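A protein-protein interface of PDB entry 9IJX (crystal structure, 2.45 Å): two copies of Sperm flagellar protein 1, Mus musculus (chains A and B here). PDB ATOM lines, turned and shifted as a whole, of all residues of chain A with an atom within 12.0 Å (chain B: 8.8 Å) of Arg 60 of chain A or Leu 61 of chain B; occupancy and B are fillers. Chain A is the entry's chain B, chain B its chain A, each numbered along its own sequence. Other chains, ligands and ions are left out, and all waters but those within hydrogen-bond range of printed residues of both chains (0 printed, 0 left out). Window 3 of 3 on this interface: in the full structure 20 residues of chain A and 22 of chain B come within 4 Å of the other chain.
Lys 50 of chain A touches Ile 54 of chain B.
Ile 54 of chain B touches Arg 53 of chain A.
Ile 54 of chain B touches Ile 54 of chain A.
Leu 57 of chain A touches Leu 61 of chain B (CD1 to CD2, 3.9 Å).
Arg 60 of chain A touches Leu 61 of chain B (O to CD1, 3.4 Å).
Leu 61 of chain A touches Leu 57 of chain B.
Leu 61 of chain A touches Arg 60 of chain B.
N of Leu 61 of chain B touches CD1 of Leu 61 of chain A, at 3.7 Å.
Printed residues of chain B that touch a printed residue of chain A: Ile 54, Leu 57, Arg 60 and Leu 61.
Among the printed residues, 8 pairs touch across the chains.
Among the printed residues, no Asp or Glu carboxylate lies within 4 Å of a Lys or Arg side-chain nitrogen of the other chain.
Arg 60 of chain A touches just one residue of chain B: Leu 61.
Leu 61 of chain B touches three residues of chain A.
No residue of chain A comes within 4 Å of Ser 58 of chain B.
No residue of chain A comes within 4 Å of Gln 62 of chain B.
Of the printed residues of chain B, Lys 50 of chain A touches Ile 54.
Of the printed residues of chain B, Leu 61 of chain A touches Leu 57, Arg 60 and Leu 61.
Of the printed residues of chain B, Arg 53 of chain A touches Ile 54.
Printed residues of chain B within 4 Å of Ile 54 of chain A: Ile 54 (3.5 Å).
Ser 58 of chain A touches none of the printed residues of chain B.
NH1 of Arg 60 of chain B is in salt-bridge range of OD2 of Asp 56 of chain B, at 3.7 Å.
OD2 of Asp 56 of chain A is in salt-bridge range of NH1 of Arg 60 of chain A, 3.8 Å away.
Ile 54 of chain B touches its own counterpart, Ile 54 of chain A.
Leu 57 of chain A touches Leu 61 of chain B, and with the chains exchanged Leu 61 of chain A touches Leu 57 of chain B.
Arg 60 of chain A touches Leu 61 of chain B, and with the chains exchanged Leu 61 of chain A touches Arg 60 of chain B.
Leu 61 of chain A touches its own counterpart, Leu 61 of chain B.
Positions printed for both chains: 54, 55, 56, 57, 58, 59, 60, 61 and 62.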
ATOM      1  N   LYS A  50      -8.877  -5.058  18.607  1.00  0.00           N
ATOM      2  CA  LYS A  50      -8.262  -5.233  19.953  1.00  0.00           C
ATOM      3  C   LYS A  50      -9.290  -4.897  21.037  1.00  0.00           C
ATOM      4  O   LYS A  50      -9.300  -5.574  22.062  1.00  0.00           O
ATOM      5  CB  LYS A  50      -6.996  -4.386  20.087  1.00  0.00           C
ATOM      6  CG  LYS A  50      -5.905  -4.761  19.077  1.00  0.00           C
ATOM      7  CD  LYS A  50      -5.366  -6.180  19.215  1.00  0.00           C
ATOM      8  CE  LYS A  50      -5.253  -6.929  17.897  1.00  0.00           C
ATOM      9  NZ  LYS A  50      -5.207  -8.395  18.107  1.00  0.00           N
ATOM     10  N   ASN A  51     -10.134  -3.894  20.821  1.00  0.00           N
ATOM     11  CA  ASN A  51     -11.204  -3.517  21.783  1.00  0.00           C
ATOM     12  C   ASN A  51     -12.206  -4.668  21.934  1.00  0.00           C
ATOM     13  O   ASN A  51     -12.673  -4.889  23.067  1.00  0.00           O
ATOM     14  CB  ASN A  51     -11.871  -2.202  21.385  1.00  0.00           C
ATOM     15  CG  ASN A  51     -11.002  -1.019  21.737  1.00  0.00           C
ATOM     16  OD1 ASN A  51     -10.150  -1.123  22.617  1.00  0.00           O
ATOM     17  ND2 ASN A  51     -11.212   0.101  21.066  1.00  0.00           N
ATOM     18  N   VAL A  52     -12.507  -5.389  20.855  1.00  0.00           N
ATOM     19  CA  VAL A  52     -13.431  -6.564  20.879  1.00  0.00           C
ATOM     20  C   VAL A  52     -12.780  -7.700  21.682  1.00  0.00           C
ATOM     21  O   VAL A  52     -13.479  -8.289  22.536  1.00  0.00           O
ATOM     22  CB  VAL A  52     -13.824  -7.014  19.455  1.00  0.00           C
ATOM     23  CG1 VAL A  52     -14.347  -8.446  19.417  1.00  0.00           C
ATOM     24  CG2 VAL A  52     -14.812  -6.053  18.821  1.00  0.00           C
ATOM     25  N   ARG A  53     -11.500  -8.002  21.421  1.00  0.00           N
ATOM     26  CA  ARG A  53     -10.713  -9.020  22.169  1.00  0.00           C
ATOM     27  C   ARG A  53     -10.752  -8.680  23.673  1.00  0.00           C
ATOM     28  O   ARG A  53     -10.965  -9.601  24.481  1.00  0.00           O
ATOM     29  CB  ARG A  53      -9.272  -9.088  21.648  1.00  0.00           C
ATOM     30  CG  ARG A  53      -8.939 -10.252  20.717  1.00  0.00           C
ATOM     31  CD  ARG A  53      -7.497 -10.162  20.248  1.00  0.00           C
ATOM     32  NE  ARG A  53      -6.807 -11.448  20.125  1.00  0.00           N
ATOM     33  CZ  ARG A  53      -5.483 -11.627  20.204  1.00  0.00           C
ATOM     34  NH1 ARG A  53      -4.662 -10.606  20.407  1.00  0.00           N
ATOM     35  NH2 ARG A  53      -4.975 -12.843  20.081  1.00  0.00           N
ATOM     36  N   ILE A  54     -10.565  -7.403  24.022  1.00  0.00           N
ATOM     37  CA  ILE A  54     -10.555  -6.909  25.433  1.00  0.00           C
ATOM     38  C   ILE A  54     -11.932  -7.161  26.062  1.00  0.00           C
ATOM     39  O   ILE A  54     -11.972  -7.645  27.211  1.00  0.00           O
ATOM     40  CB  ILE A  54     -10.143  -5.420  25.500  1.00  0.00           C
ATOM     41  CG1 ILE A  54      -8.641  -5.253  25.253  1.00  0.00           C
ATOM     42  CG2 ILE A  54     -10.568  -4.786  26.818  1.00  0.00           C
ATOM     43  CD1 ILE A  54      -8.195  -3.827  24.992  1.00  0.00           C
ATOM     44  N   ASP A  55     -13.012  -6.853  25.338  1.00  0.00           N
ATOM     45  CA  ASP A  55     -14.415  -7.002  25.811  1.00  0.00           C
ATOM     46  C   ASP A  55     -14.759  -8.484  25.948  1.00  0.00           C
ATOM     47  O   ASP A  55     -15.441  -8.829  26.928  1.00  0.00           O
ATOM     48  CB  ASP A  55     -15.398  -6.299  24.871  1.00  0.00           C
ATOM     49  CG  ASP A  55     -15.237  -4.791  24.869  1.00  0.00           C
ATOM     50  OD1 ASP A  55     -14.546  -4.275  25.779  1.00  0.00           O
ATOM     51  OD2 ASP A  55     -15.768  -4.151  23.940  1.00  0.00           O
ATOM     52  N   ASP A  56     -14.311  -9.313  25.000  1.00  0.00           N
ATOM     53  CA  ASP A  56     -14.428 -10.795  25.075  1.00  0.00           C
ATOM     54  C   ASP A  56     -13.774 -11.273  26.379  1.00  0.00           C
ATOM     55  O   ASP A  56     -14.508 -11.786  27.257  1.00  0.00           O
ATOM     56  CB  ASP A  56     -13.807 -11.472  23.851  1.00  0.00           C
ATOM     57  CG  ASP A  56     -13.814 -12.995  23.921  1.00  0.00           C
ATOM     58  OD1 ASP A  56     -14.825 -13.563  24.404  1.00  0.00           O
ATOM     59  OD2 ASP A  56     -12.805 -13.608  23.498  1.00  0.00           O
ATOM     60  N   LEU A  57     -12.452 -11.086  26.501  1.00  0.00           N
ATOM     61  CA  LEU A  57     -11.635 -11.546  27.658  1.00  0.00           C
ATOM     62  C   LEU A  57     -12.254 -11.028  28.965  1.00  0.00           C
ATOM     63  O   LEU A  57     -12.333 -11.810  29.928  1.00  0.00           O
ATOM     64  CB  LEU A  57     -10.190 -11.060  27.504  1.00  0.00           C
ATOM     65  CG  LEU A  57      -9.241 -11.959  26.699  1.00  0.00           C
ATOM     66  CD1 LEU A  57      -9.277 -13.405  27.183  1.00  0.00           C
ATOM     67  CD2 LEU A  57      -9.530 -11.903  25.207  1.00  0.00           C
ATOM     68  N   SER A  58     -12.680  -9.760  28.988  1.00  0.00           N
ATOM     69  CA  SER A  58     -13.264  -9.074  30.172  1.00  0.00           C
ATOM     70  C   SER A  58     -14.573  -9.763  30.595  1.00  0.00           C
ATOM     71  O   SER A  58     -14.717 -10.064  31.794  1.00  0.00           O
ATOM     72  CB  SER A  58     -13.458  -7.601  29.899  1.00  0.00           C
ATOM     73  OG  SER A  58     -14.263  -7.003  30.896  1.00  0.00           O
ATOM     74  N   ARG A  59     -15.490 -10.013  29.649  1.00  0.00           N
ATOM     75  CA  ARG A  59     -16.774 -10.735  29.884  1.00  0.00           C
ATOM     76  C   ARG A  59     -16.470 -12.113  30.477  1.00  0.00           C
ATOM     77  O   ARG A  59     -17.105 -12.480  31.477  1.00  0.00           O
ATOM     78  CB  ARG A  59     -17.575 -10.859  28.583  1.00  0.00           C
ATOM     79  CG  ARG A  59     -18.869 -11.655  28.669  1.00  0.00           C
ATOM     80  CD  ARG A  59     -19.487 -11.855  27.306  1.00  0.00           C
ATOM     81  NE  ARG A  59     -19.791 -10.557  26.709  1.00  0.00           N
ATOM     82  CZ  ARG A  59     -20.517 -10.354  25.612  1.00  0.00           C
ATOM     83  NH1 ARG A  59     -21.046 -11.367  24.939  1.00  0.00           N
ATOM     84  NH2 ARG A  59     -20.718  -9.118  25.178  1.00  0.00           N
ATOM     85  N   ARG A  60     -15.530 -12.847  29.879  1.00  0.00           N
ATOM     86  CA  ARG A  60     -15.154 -14.227  30.298  1.00  0.00           C
ATOM     87  C   ARG A  60     -14.473 -14.206  31.674  1.00  0.00           C
ATOM     88  O   ARG A  60     -14.389 -15.270  32.301  1.00  0.00           O
ATOM     89  CB  ARG A  60     -14.242 -14.864  29.249  1.00  0.00           C
ATOM     90  CG  ARG A  60     -14.956 -15.189  27.944  1.00  0.00           C
ATOM     91  CD  ARG A  60     -14.001 -15.599  26.850  1.00  0.00           C
ATOM     92  NE  ARG A  60     -13.192 -16.742  27.250  1.00  0.00           N
ATOM     93  CZ  ARG A  60     -12.197 -17.257  26.544  1.00  0.00           C
ATOM     94  NH1 ARG A  60     -11.867 -16.747  25.366  1.00  0.00           N
ATOM     95  NH2 ARG A  60     -11.533 -18.301  27.016  1.00  0.00           N
ATOM     96  N   LEU A  61     -13.975 -13.046  32.111  1.00  0.00           N
ATOM     97  CA  LEU A  61     -13.376 -12.852  33.459  1.00  0.00           C
ATOM     98  C   LEU A  61     -14.490 -12.669  34.497  1.00  0.00           C
ATOM     99  O   LEU A  61     -14.347 -13.209  35.613  1.00  0.00           O
ATOM    100  CB  LEU A  61     -12.437 -11.641  33.439  1.00  0.00           C
ATOM    101  CG  LEU A  61     -11.666 -11.405  34.739  1.00  0.00           C
ATOM    102  CD1 LEU A  61     -10.651 -12.515  34.993  1.00  0.00           C
ATOM    103  CD2 LEU A  61     -10.970 -10.053  34.714  1.00  0.00           C
ATOM    104  N   GLN A  62     -15.530 -11.900  34.152  1.00  0.00           N
ATOM    105  CA  GLN A  62     -16.737 -11.662  34.996  1.00  0.00           C
ATOM    106  C   GLN A  62     -17.414 -13.005  35.299  1.00  0.00           C
ATOM    107  O   GLN A  62     -18.082 -13.092  36.348  1.00  0.00           O
ATOM    108  CB  GLN A  62     -17.664 -10.654  34.305  1.00  0.00           C
ATOM    109  CG  GLN A  62     -19.130 -10.698  34.723  1.00  0.00           C
ATOM    110  CD  GLN A  62     -20.030 -10.232  33.603  1.00  0.00           C
ATOM    111  OE1 GLN A  62     -20.194  -9.036  33.361  1.00  0.00           O
ATOM    112  NE2 GLN A  62     -20.625 -11.186  32.904  1.00  0.00           N
ATOM    113  N   GLN A  63     -17.233 -14.013  34.435  1.00  0.00           N
ATOM    114  CA  GLN A  63     -17.550 -15.442  34.733  1.00  0.00           C
ATOM    115  C   GLN A  63     -16.475 -16.025  35.666  1.00  0.00           C
ATOM    116  O   GLN A  63     -15.737 -16.951  35.244  1.00  0.00           O
ATOM    117  CB  GLN A  63     -17.660 -16.241  33.431  1.00  0.00           C
ATOM    118  CG  GLN A  63     -18.780 -15.777  32.515  1.00  0.00           C
ATOM    119  CD  GLN A  63     -18.497 -16.003  31.046  1.00  0.00           C
ATOM    120  OE1 GLN A  63     -17.858 -16.974  30.637  1.00  0.00           O
ATOM    121  NE2 GLN A  63     -18.986 -15.090  30.227  1.00  0.00           N
ATOM    122  N   ALA A  64     -16.411 -15.499  36.896  1.00  0.00           N
ATOM    123  CA  ALA A  64     -15.515 -15.923  37.999  1.00  0.00           C
ATOM    124  C   ALA A  64     -16.352 -16.163  39.262  1.00  0.00           C
ATOM    125  O   ALA A  64     -17.225 -15.357  39.598  1.00  0.00           O
ATOM    126  CB  ALA A  64     -14.456 -14.872  38.242  1.00  0.00           C
ATOM    127  N   ILE B  54      -4.813  -6.855  27.064  1.00  0.00           N
ATOM    128  CA  ILE B  54      -5.274  -8.210  26.624  1.00  0.00           C
ATOM    129  C   ILE B  54      -4.512  -9.283  27.418  1.00  0.00           C
ATOM    130  O   ILE B  54      -5.159 -10.236  27.898  1.00  0.00           O
ATOM    131  CB  ILE B  54      -5.119  -8.383  25.099  1.00  0.00           C
ATOM    132  CG1 ILE B  54      -6.174  -7.578  24.333  1.00  0.00           C
ATOM    133  CG2 ILE B  54      -5.137  -9.855  24.707  1.00  0.00           C
ATOM    134  CD1 ILE B  54      -5.903  -7.432  22.850  1.00  0.00           C
ATOM    135  N   ASP B  55      -3.193  -9.128  27.554  1.00  0.00           N
ATOM    136  CA  ASP B  55      -2.302 -10.089  28.262  1.00  0.00           C
ATOM    137  C   ASP B  55      -2.606 -10.065  29.767  1.00  0.00           C
ATOM    138  O   ASP B  55      -2.604 -11.143  30.386  1.00  0.00           O
ATOM    139  CB  ASP B  55      -0.830  -9.778  27.994  1.00  0.00           C
ATOM    140  CG  ASP B  55      -0.433  -9.981  26.542  1.00  0.00           C
ATOM    141  OD1 ASP B  55      -1.219 -10.618  25.805  1.00  0.00           O
ATOM    142  OD2 ASP B  55       0.642  -9.471  26.146  1.00  0.00           O
ATOM    143  N   ASP B  56      -2.843  -8.881  30.329  1.00  0.00           N
ATOM    144  CA  ASP B  56      -3.304  -8.701  31.731  1.00  0.00           C
ATOM    145  C   ASP B  56      -4.602  -9.494  31.932  1.00  0.00           C
ATOM    146  O   ASP B  56      -4.581 -10.464  32.711  1.00  0.00           O
ATOM    147  CB  ASP B  56      -3.490  -7.220  32.070  1.00  0.00           C
ATOM    148  CG  ASP B  56      -4.057  -6.959  33.450  1.00  0.00           C
ATOM    149  OD1 ASP B  56      -3.670  -7.681  34.399  1.00  0.00           O
ATOM    150  OD2 ASP B  56      -4.880  -6.029  33.563  1.00  0.00           O
ATOM    151  N   LEU B  57      -5.673  -9.112  31.230  1.00  0.00           N
ATOM    152  CA  LEU B  57      -7.029  -9.729  31.335  1.00  0.00           C
ATOM    153  C   LEU B  57      -6.920 -11.245  31.133  1.00  0.00           C
ATOM    154  O   LEU B  57      -7.569 -11.979  31.891  1.00  0.00           O
ATOM    155  CB  LEU B  57      -7.974  -9.107  30.299  1.00  0.00           C
ATOM    156  CG  LEU B  57      -8.714  -7.831  30.718  1.00  0.00           C
ATOM    157  CD1 LEU B  57      -9.424  -8.004  32.054  1.00  0.00           C
ATOM    158  CD2 LEU B  57      -7.789  -6.623  30.776  1.00  0.00           C
ATOM    159  N   SER B  58      -6.126 -11.689  30.153  1.00  0.00           N
ATOM    160  CA  SER B  58      -5.928 -13.119  29.793  1.00  0.00           C
ATOM    161  C   SER B  58      -5.294 -13.883  30.969  1.00  0.00           C
ATOM    162  O   SER B  58      -5.828 -14.954  31.334  1.00  0.00           O
ATOM    163  CB  SER B  58      -5.118 -13.246  28.526  1.00  0.00           C
ATOM    164  OG  SER B  58      -4.702 -14.582  28.329  1.00  0.00           O
ATOM    165  N   ARG B  59      -4.213 -13.350  31.553  1.00  0.00           N
ATOM    166  CA  ARG B  59      -3.529 -13.922  32.749  1.00  0.00           C
ATOM    167  C   ARG B  59      -4.543 -14.054  33.892  1.00  0.00           C
ATOM    168  O   ARG B  59      -4.604 -15.134  34.504  1.00  0.00           O
ATOM    169  CB  ARG B  59      -2.334 -13.059  33.182  1.00  0.00           C
ATOM    170  CG  ARG B  59      -0.989 -13.544  32.667  1.00  0.00           C
ATOM    171  CD  ARG B  59       0.146 -12.639  33.113  1.00  0.00           C
ATOM    172  NE  ARG B  59       1.449 -13.020  32.570  1.00  0.00           N
ATOM    173  CZ  ARG B  59       2.276 -13.946  33.075  1.00  0.00           C
ATOM    174  NH1 ARG B  59       1.945 -14.639  34.154  1.00  0.00           N
ATOM    175  NH2 ARG B  59       3.437 -14.183  32.485  1.00  0.00           N
ATOM    176  N   ARG B  60      -5.309 -12.994  34.157  1.00  0.00           N
ATOM    177  CA  ARG B  60      -6.300 -12.932  35.265  1.00  0.00           C
ATOM    178  C   ARG B  60      -7.463 -13.897  35.004  1.00  0.00           C
ATOM    179  O   ARG B  60      -8.174 -14.218  35.980  1.00  0.00           O
ATOM    180  CB  ARG B  60      -6.818 -11.502  35.439  1.00  0.00           C
ATOM    181  CG  ARG B  60      -5.787 -10.537  36.003  1.00  0.00           C
ATOM    182  CD  ARG B  60      -6.242  -9.097  35.890  1.00  0.00           C
ATOM    183  NE  ARG B  60      -7.538  -8.823  36.491  1.00  0.00           N
ATOM    184  CZ  ARG B  60      -8.400  -7.899  36.063  1.00  0.00           C
ATOM    185  NH1 ARG B  60      -8.148  -7.181  34.979  1.00  0.00           N
ATOM    186  NH2 ARG B  60      -9.539  -7.717  36.708  1.00  0.00           N
ATOM    187  N   LEU B  61      -7.653 -14.333  33.751  1.00  0.00           N
ATOM    188  CA  LEU B  61      -8.676 -15.344  33.360  1.00  0.00           C
ATOM    189  C   LEU B  61      -8.178 -16.750  33.748  1.00  0.00           C
ATOM    190  O   LEU B  61      -9.028 -17.560  34.173  1.00  0.00           O
ATOM    191  CB  LEU B  61      -8.973 -15.200  31.860  1.00  0.00           C
ATOM    192  CG  LEU B  61      -9.767 -16.311  31.177  1.00  0.00           C
ATOM    193  CD1 LEU B  61     -11.243 -16.119  31.444  1.00  0.00           C
ATOM    194  CD2 LEU B  61      -9.467 -16.367  29.686  1.00  0.00           C
ATOM    195  N   GLN B  62      -6.866 -17.013  33.718  1.00  0.00           N
ATOM    196  CA  GLN B  62      -6.286 -18.310  34.173  1.00  0.00           C
ATOM    197  C   GLN B  62      -6.335 -18.393  35.707  1.00  0.00           C
ATOM    198  O   GLN B  62      -6.192 -17.425  36.459  1.00  0.00           O
ATOM    199  CB  GLN B  62      -4.860 -18.487  33.648  1.00  0.00           C
ATOM    200  CG  GLN B  62      -4.776 -18.554  32.130  1.00  0.00           C
ATOM    201  CD  GLN B  62      -3.376 -18.835  31.638  1.00  0.00           C
ATOM    202  OE1 GLN B  62      -2.750 -18.003  30.981  1.00  0.00           O
ATOM    203  NE2 GLN B  62      -2.870 -20.017  31.957  1.00  0.00           N
